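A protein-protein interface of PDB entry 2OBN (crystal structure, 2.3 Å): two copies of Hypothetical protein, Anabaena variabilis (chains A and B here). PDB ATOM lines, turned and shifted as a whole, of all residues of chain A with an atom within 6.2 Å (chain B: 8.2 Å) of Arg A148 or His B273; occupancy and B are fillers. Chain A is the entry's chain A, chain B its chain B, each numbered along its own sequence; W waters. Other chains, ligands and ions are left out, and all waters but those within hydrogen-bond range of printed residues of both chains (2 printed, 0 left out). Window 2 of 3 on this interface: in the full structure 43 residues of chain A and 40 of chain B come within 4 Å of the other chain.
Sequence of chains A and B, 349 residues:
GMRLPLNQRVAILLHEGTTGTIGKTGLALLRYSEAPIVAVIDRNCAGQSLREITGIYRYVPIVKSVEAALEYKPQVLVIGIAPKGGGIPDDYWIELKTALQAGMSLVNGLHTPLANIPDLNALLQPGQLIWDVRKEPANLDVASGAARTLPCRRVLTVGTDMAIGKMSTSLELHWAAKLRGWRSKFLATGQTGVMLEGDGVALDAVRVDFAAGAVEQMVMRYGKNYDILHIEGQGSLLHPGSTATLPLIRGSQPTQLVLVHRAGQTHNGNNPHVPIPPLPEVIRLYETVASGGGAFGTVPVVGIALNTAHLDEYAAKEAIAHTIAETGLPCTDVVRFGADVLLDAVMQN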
ATOM      1  N   SER A 144     -23.839  16.734  25.219  1.00  0.00           N
ATOM      2  CA  SER A 144     -24.782  15.849  25.905  1.00  0.00           C
ATOM      3  C   SER A 144     -25.485  16.497  27.099  1.00  0.00           C
ATOM      4  O   SER A 144     -26.000  15.788  27.983  1.00  0.00           O
ATOM      5  CB  SER A 144     -23.993  14.661  26.429  1.00  0.00           C
ATOM      6  OG  SER A 144     -22.954  15.143  27.256  1.00  0.00           O
ATOM      7  N   GLY A 145     -25.519  17.822  27.130  1.00  0.00           N
ATOM      8  CA  GLY A 145     -26.141  18.553  28.234  1.00  0.00           C
ATOM      9  C   GLY A 145     -25.408  18.427  29.548  1.00  0.00           C
ATOM     10  O   GLY A 145     -26.007  18.573  30.590  1.00  0.00           O
ATOM     11  N   ALA A 146     -24.102  18.179  29.498  1.00  0.00           N
ATOM     12  CA  ALA A 146     -23.298  17.992  30.711  1.00  0.00           C
ATOM     13  C   ALA A 146     -23.178  19.253  31.569  1.00  0.00           C
ATOM     14  O   ALA A 146     -23.037  19.176  32.792  1.00  0.00           O
ATOM     15  CB  ALA A 146     -21.920  17.479  30.336  1.00  0.00           C
ATOM     16  N   ALA A 147     -23.240  20.412  30.930  1.00  0.00           N
ATOM     17  CA  ALA A 147     -23.138  21.677  31.652  1.00  0.00           C
ATOM     18  C   ALA A 147     -24.225  21.881  32.718  1.00  0.00           C
ATOM     19  O   ALA A 147     -24.012  22.629  33.675  1.00  0.00           O
ATOM     20  CB  ALA A 147     -23.156  22.817  30.680  1.00  0.00           C
ATOM     21  N   ARG A 148     -25.370  21.216  32.559  1.00  0.00           N
ATOM     22  CA  ARG A 148     -26.478  21.338  33.511  1.00  0.00           C
ATOM     23  C   ARG A 148     -26.108  20.856  34.917  1.00  0.00           C
ATOM     24  O   ARG A 148     -26.735  21.261  35.893  1.00  0.00           O
ATOM     25  CB  ARG A 148     -27.696  20.548  33.021  1.00  0.00           C
ATOM     26  CG  ARG A 148     -27.643  19.058  33.308  1.00  0.00           C
ATOM     27  CD  ARG A 148     -28.693  18.308  32.510  1.00  0.00           C
ATOM     28  NE  ARG A 148     -28.942  17.010  33.119  1.00  0.00           N
ATOM     29  CZ  ARG A 148     -28.170  15.935  32.991  1.00  0.00           C
ATOM     30  NH1 ARG A 148     -27.063  15.963  32.259  1.00  0.00           N
ATOM     31  NH2 ARG A 148     -28.524  14.817  33.606  1.00  0.00           N
ATOM     32  N   THR A 149     -25.101  19.991  35.004  1.00  0.00           N
ATOM     33  CA  THR A 149     -24.644  19.448  36.269  1.00  0.00           C
ATOM     34  C   THR A 149     -23.704  20.376  37.054  1.00  0.00           C
ATOM     35  O   THR A 149     -23.391  20.087  38.209  1.00  0.00           O
ATOM     36  CB  THR A 149     -23.902  18.119  36.044  1.00  0.00           C
ATOM     37  OG1 THR A 149     -22.706  18.359  35.301  1.00  0.00           O
ATOM     38  CG2 THR A 149     -24.769  17.142  35.267  1.00  0.00           C
ATOM     39  N   LEU A 150     -23.255  21.479  36.454  1.00  0.00           N
ATOM     40  CA  LEU A 150     -22.316  22.385  37.138  1.00  0.00           C
ATOM     41  C   LEU A 150     -23.027  23.237  38.191  1.00  0.00           C
ATOM     42  O   LEU A 150     -24.141  23.691  37.969  1.00  0.00           O
ATOM     43  CB  LEU A 150     -21.585  23.277  36.124  1.00  0.00           C
ATOM     44  CG  LEU A 150     -20.699  22.550  35.092  1.00  0.00           C
ATOM     45  CD1 LEU A 150     -20.334  23.466  33.962  1.00  0.00           C
ATOM     46  CD2 LEU A 150     -19.449  21.958  35.726  1.00  0.00           C
ATOM     47  N   PRO A 151     -22.382  23.447  39.348  1.00  0.00           N
ATOM     48  CA  PRO A 151     -22.972  24.219  40.447  1.00  0.00           C
ATOM     49  C   PRO A 151     -22.977  25.735  40.250  1.00  0.00           C
ATOM     50  O   PRO A 151     -23.650  26.439  40.996  1.00  0.00           O
ATOM     51  CB  PRO A 151     -22.077  23.866  41.627  1.00  0.00           C
ATOM     52  CG  PRO A 151     -20.746  23.646  41.020  1.00  0.00           C
ATOM     53  CD  PRO A 151     -21.030  22.967  39.692  1.00  0.00           C
ATOM     54  N   ARG A 154     -24.539  30.154  34.858  1.00  0.00           N
ATOM     55  CA  ARG A 154     -24.041  30.249  33.497  1.00  0.00           C
ATOM     56  C   ARG A 154     -24.924  31.266  32.789  1.00  0.00           C
ATOM     57  O   ARG A 154     -26.057  30.963  32.405  1.00  0.00           O
ATOM     58  CB  ARG A 154     -24.054  28.869  32.842  1.00  0.00           C
ATOM     59  CG  ARG A 154     -23.174  27.883  33.601  1.00  0.00           C
ATOM     60  CD  ARG A 154     -23.285  26.468  33.120  1.00  0.00           C
ATOM     61  NE  ARG A 154     -24.635  25.903  33.225  1.00  0.00           N
ATOM     62  CZ  ARG A 154     -25.182  25.409  34.333  1.00  0.00           C
ATOM     63  NH1 ARG A 154     -24.539  25.444  35.489  1.00  0.00           N
ATOM     64  NH2 ARG A 154     -26.405  24.887  34.290  1.00  0.00           N
ATOM     65  N   MET A 220     -17.246  23.133  30.746  1.00  0.00           N
ATOM     66  CA  MET A 220     -16.861  22.081  31.676  1.00  0.00           C
ATOM     67  C   MET A 220     -15.454  22.318  32.221  1.00  0.00           C
ATOM     68  O   MET A 220     -15.195  21.997  33.371  1.00  0.00           O
ATOM     69  CB  MET A 220     -17.000  20.701  31.016  1.00  0.00           C
ATOM     70  CG  MET A 220     -18.457  20.362  30.605  1.00  0.00           C
ATOM     71  SD  MET A 220     -19.674  20.287  32.098  1.00  0.00           S
ATOM     72  CE  MET A 220     -19.025  18.676  32.910  1.00  0.00           C
ATOM     73  N   SER A 252     -23.923  25.369  26.763  1.00  0.00           N
ATOM     74  CA  SER A 252     -23.722  25.953  28.080  1.00  0.00           C
ATOM     75  C   SER A 252     -24.856  25.676  29.070  1.00  0.00           C
ATOM     76  O   SER A 252     -24.651  25.874  30.265  1.00  0.00           O
ATOM     77  CB  SER A 252     -23.496  27.453  27.964  1.00  0.00           C
ATOM     78  OG  SER A 252     -24.687  28.101  27.608  1.00  0.00           O
ATOM     79  N   GLN A 253     -26.030  25.231  28.599  1.00  0.00           N
ATOM     80  CA  GLN A 253     -27.153  24.945  29.490  1.00  0.00           C
ATOM     81  C   GLN A 253     -27.324  26.116  30.473  1.00  0.00           C
ATOM     82  O   GLN A 253     -27.297  25.931  31.681  1.00  0.00           O
ATOM     83  CB  GLN A 253     -26.893  23.632  30.235  1.00  0.00           C
ATOM     84  CG  GLN A 253     -26.767  22.396  29.290  1.00  0.00           C
ATOM     85  CD  GLN A 253     -28.121  21.848  28.837  1.00  0.00           C
ATOM     86  OE1 GLN A 253     -28.861  21.261  29.640  1.00  0.00           O
ATOM     87  NE2 GLN A 253     -28.427  21.987  27.543  1.00  0.00           N
ATOM     88  N   ALA A 295     -37.813  20.175  27.093  1.00  0.00           N
ATOM     89  CA  ALA A 295     -36.713  19.206  27.084  1.00  0.00           C
ATOM     90  C   ALA A 295     -35.583  19.608  28.059  1.00  0.00           C
ATOM     91  O   ALA A 295     -34.845  18.748  28.573  1.00  0.00           O
ATOM     92  CB  ALA A 295     -36.182  19.032  25.672  1.00  0.00           C
ATOM     93  N   PRO B 240     -29.757  17.698  22.839  1.00  0.00           N
ATOM     94  CA  PRO B 240     -28.829  18.652  23.489  1.00  0.00           C
ATOM     95  C   PRO B 240     -27.523  18.991  22.750  1.00  0.00           C
ATOM     96  O   PRO B 240     -26.833  19.937  23.132  1.00  0.00           O
ATOM     97  CB  PRO B 240     -28.487  17.951  24.812  1.00  0.00           C
ATOM     98  CG  PRO B 240     -28.716  16.527  24.550  1.00  0.00           C
ATOM     99  CD  PRO B 240     -29.863  16.450  23.621  1.00  0.00           C
ATOM    100  N   THR B 266     -40.338   8.884  24.432  1.00  0.00           N
ATOM    101  CA  THR B 266     -40.499   9.943  25.431  1.00  0.00           C
ATOM    102  C   THR B 266     -39.203  10.661  25.806  1.00  0.00           C
ATOM    103  O   THR B 266     -39.242  11.693  26.462  1.00  0.00           O
ATOM    104  CB  THR B 266     -41.170   9.381  26.712  1.00  0.00           C
ATOM    105  OG1 THR B 266     -40.351   8.355  27.294  1.00  0.00           O
ATOM    106  CG2 THR B 266     -42.541   8.799  26.377  1.00  0.00           C
ATOM    107  N   HIS B 267     -38.058  10.137  25.375  1.00  0.00           N
ATOM    108  CA  HIS B 267     -36.769  10.728  25.719  1.00  0.00           C
ATOM    109  C   HIS B 267     -35.810  10.636  24.542  1.00  0.00           C
ATOM    110  O   HIS B 267     -35.953   9.775  23.663  1.00  0.00           O
ATOM    111  CB  HIS B 267     -36.153   9.991  26.923  1.00  0.00           C
ATOM    112  CG  HIS B 267     -36.952  10.084  28.192  1.00  0.00           C
ATOM    113  ND1 HIS B 267     -37.967   9.200  28.505  1.00  0.00           N
ATOM    114  CD2 HIS B 267     -36.864  10.939  29.241  1.00  0.00           C
ATOM    115  CE1 HIS B 267     -38.477   9.518  29.682  1.00  0.00           C
ATOM    116  NE2 HIS B 267     -37.822  10.565  30.153  1.00  0.00           N
ATOM    117  N   ASN B 268     -34.836  11.544  24.517  1.00  0.00           N
ATOM    118  CA  ASN B 268     -33.807  11.557  23.487  1.00  0.00           C
ATOM    119  C   ASN B 268     -33.108  10.186  23.496  1.00  0.00           C
ATOM    120  O   ASN B 268     -32.925   9.578  24.557  1.00  0.00           O
ATOM    121  CB  ASN B 268     -32.818  12.672  23.806  1.00  0.00           C
ATOM    122  CG  ASN B 268     -31.740  12.823  22.768  1.00  0.00           C
ATOM    123  OD1 ASN B 268     -30.585  12.519  23.032  1.00  0.00           O
ATOM    124  ND2 ASN B 268     -32.108  13.303  21.576  1.00  0.00           N
ATOM    125  N   GLY B 269     -32.760   9.680  22.327  1.00  0.00           N
ATOM    126  CA  GLY B 269     -32.098   8.390  22.228  1.00  0.00           C
ATOM    127  C   GLY B 269     -30.673   8.380  22.742  1.00  0.00           C
ATOM    128  O   GLY B 269     -30.311   7.521  23.546  1.00  0.00           O
ATOM    129  N   ASN B 270     -29.862   9.325  22.273  1.00  0.00           N
ATOM    130  CA  ASN B 270     -28.473   9.416  22.717  1.00  0.00           C
ATOM    131  C   ASN B 270     -28.318   9.879  24.158  1.00  0.00           C
ATOM    132  O   ASN B 270     -27.386   9.456  24.826  1.00  0.00           O
ATOM    133  CB  ASN B 270     -27.665  10.381  21.842  1.00  0.00           C
ATOM    134  CG  ASN B 270     -27.540   9.923  20.402  1.00  0.00           C
ATOM    135  OD1 ASN B 270     -27.326  10.752  19.501  1.00  0.00           O
ATOM    136  ND2 ASN B 270     -27.687   8.615  20.164  1.00  0.00           N
ATOM    137  N   ASN B 271     -29.211  10.764  24.606  1.00  0.00           N
ATOM    138  CA  ASN B 271     -29.168  11.358  25.955  1.00  0.00           C
ATOM    139  C   ASN B 271     -30.517  11.121  26.671  1.00  0.00           C
ATOM    140  O   ASN B 271     -31.331  12.035  26.804  1.00  0.00           O
ATOM    141  CB  ASN B 271     -28.862  12.850  25.811  1.00  0.00           C
ATOM    142  CG  ASN B 271     -27.630  13.119  24.938  1.00  0.00           C
ATOM    143  OD1 ASN B 271     -26.512  13.014  25.398  1.00  0.00           O
ATOM    144  ND2 ASN B 271     -27.850  13.485  23.682  1.00  0.00           N
ATOM    145  N   PRO B 272     -30.746   9.886  27.163  1.00  0.00           N
ATOM    146  CA  PRO B 272     -32.026   9.455  27.752  1.00  0.00           C
ATOM    147  C   PRO B 272     -32.595  10.272  28.905  1.00  0.00           C
ATOM    148  O   PRO B 272     -33.755  10.080  29.250  1.00  0.00           O
ATOM    149  CB  PRO B 272     -31.732   8.041  28.239  1.00  0.00           C
ATOM    150  CG  PRO B 272     -30.584   7.586  27.490  1.00  0.00           C
ATOM    151  CD  PRO B 272     -29.761   8.792  27.180  1.00  0.00           C
ATOM    152  N   HIS B 273     -31.795  11.150  29.499  1.00  0.00           N
ATOM    153  CA  HIS B 273     -32.258  12.007  30.590  1.00  0.00           C
ATOM    154  C   HIS B 273     -33.115  13.165  30.078  1.00  0.00           C
ATOM    155  O   HIS B 273     -33.906  13.721  30.833  1.00  0.00           O
ATOM    156  CB  HIS B 273     -31.065  12.555  31.386  1.00  0.00           C
ATOM    157  CG  HIS B 273     -30.219  13.537  30.631  1.00  0.00           C
ATOM    158  ND1 HIS B 273     -29.191  13.150  29.798  1.00  0.00           N
ATOM    159  CD2 HIS B 273     -30.249  14.891  30.589  1.00  0.00           C
ATOM    160  CE1 HIS B 273     -28.619  14.224  29.284  1.00  0.00           C
ATOM    161  NE2 HIS B 273     -29.243  15.293  29.745  1.00  0.00           N
ATOM    162  N   VAL B 274     -32.968  13.501  28.793  1.00  0.00           N
ATOM    163  CA  VAL B 274     -33.675  14.628  28.176  1.00  0.00           C
ATOM    164  C   VAL B 274     -35.036  14.198  27.672  1.00  0.00           C
ATOM    165  O   VAL B 274     -35.122  13.393  26.762  1.00  0.00           O
ATOM    166  CB  VAL B 274     -32.885  15.180  26.973  1.00  0.00           C
ATOM    167  CG1 VAL B 274     -33.585  16.399  26.385  1.00  0.00           C
ATOM    168  CG2 VAL B 274     -31.454  15.544  27.378  1.00  0.00           C
ATOM    169  N   PRO B 275     -36.115  14.727  28.255  1.00  0.00           N
ATOM    170  CA  PRO B 275     -37.404  14.309  27.706  1.00  0.00           C
ATOM    171  C   PRO B 275     -37.784  14.914  26.341  1.00  0.00           C
ATOM    172  O   PRO B 275     -37.199  15.914  25.893  1.00  0.00           O
ATOM    173  CB  PRO B 275     -38.400  14.824  28.747  1.00  0.00           C
ATOM    174  CG  PRO B 275     -37.714  15.983  29.402  1.00  0.00           C
ATOM    175  CD  PRO B 275     -36.266  15.656  29.397  1.00  0.00           C
ATOM    176  N   ILE B 276     -38.755  14.272  25.701  1.00  0.00           N
ATOM    177  CA  ILE B 276     -39.394  14.791  24.511  1.00  0.00           C
ATOM    178  C   ILE B 276     -40.697  15.391  25.017  1.00  0.00           C
ATOM    179  O   ILE B 276     -41.555  14.665  25.524  1.00  0.00           O
ATOM    180  CB  ILE B 276     -39.742  13.706  23.470  1.00  0.00           C
ATOM    181  CG1 ILE B 276     -38.457  13.063  22.917  1.00  0.00           C
ATOM    182  CG2 ILE B 276     -40.610  14.326  22.356  1.00  0.00           C
ATOM    183  CD1 ILE B 276     -38.667  12.056  21.763  1.00  0.00           C
HETATM  184  O   HOH W   1     -25.473  20.214  25.649  1.00  0.00           O
HETATM  185  O   HOH W   2     -29.864  18.521  29.132  1.00  0.00           O
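The side-chain amide oxygen (OD1) of Asn B268 sits at hydrogen-bond distance from the backbone NH (N) of Asn B271, 2.7 Å away.
O of Val B274 sits at hydrogen-bond distance from N of Asn B268 (2.9 Å).
NH1 of Arg A148 lies close to O of Gly A145 (3.3 Å).
Water W1 lies within hydrogen-bond range of N of Gly A145 (2.8 Å) and O of Pro B240 (2.9 Å).
Water W2 lies within hydrogen-bond range of the side-chain amide oxygen of Gln A253 (3.0 Å) and a ring nitrogen (NE2) of His B273 (3.3 Å).
No position is printed for both chains.
Of the 6 pairs that touch across the chains among the printed residues, none has its exchanged pair printed and touching as well.
The guanidinium group (NH1) of Arg A148 sits at hydrogen-bond distance from a ring nitrogen (NE2) of His B273 (3.4 Å).
Ser A144 touches Asn B271.
O of Ser A144 touches CE1 of His B273 (3.3 Å).
CB of Pro B240 touches N of Gly A145 (3.8 Å).
CG1 of Val B274 touches O of Ala A295, 3.4 Å away.
Ala A295 touches Pro B275.
Of the printed residues of chain B, Gly A145 touches Pro B240 (3.8 Å).
Ala A147 touches none of the printed residues of chain B.
Printed residues of chain B within 4 Å of Ala A295: Val B274 (3.4 Å) and Pro B275 (3.3 Å).
Of the printed residues of chain A, Pro B240 touches Gly A145.
Printed residues of chain A within 4 Å of Asn B271: Ser A144 (3.2 Å).
His B273 touches just these residues of chain A: Ser A144 (3.3 Å) and Arg A148 (3.3 Å).
Of the printed residues of chain A, Val B274 touches Ala A295.
The nearest residue of chain A that does not touch His B273 is Gly A145 (4.7 Å).
The nearest printed residue of chain B that does not touch Ala A295 is Ile B276 (5.4 Å).
Of the 13 printed residues of chain A, 4 touch a printed residue of chain B.
Printed residues of chain A that touch a printed residue of chain B: Ser A144, Gly A145, Arg A148 and Ala A295.
Printed residues of chain B that touch a printed residue of chain A: Pro B240, Asn B271, His B273, Val B274 and Pro B275.
Among the printed residues, 6 pairs touch across the chains.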
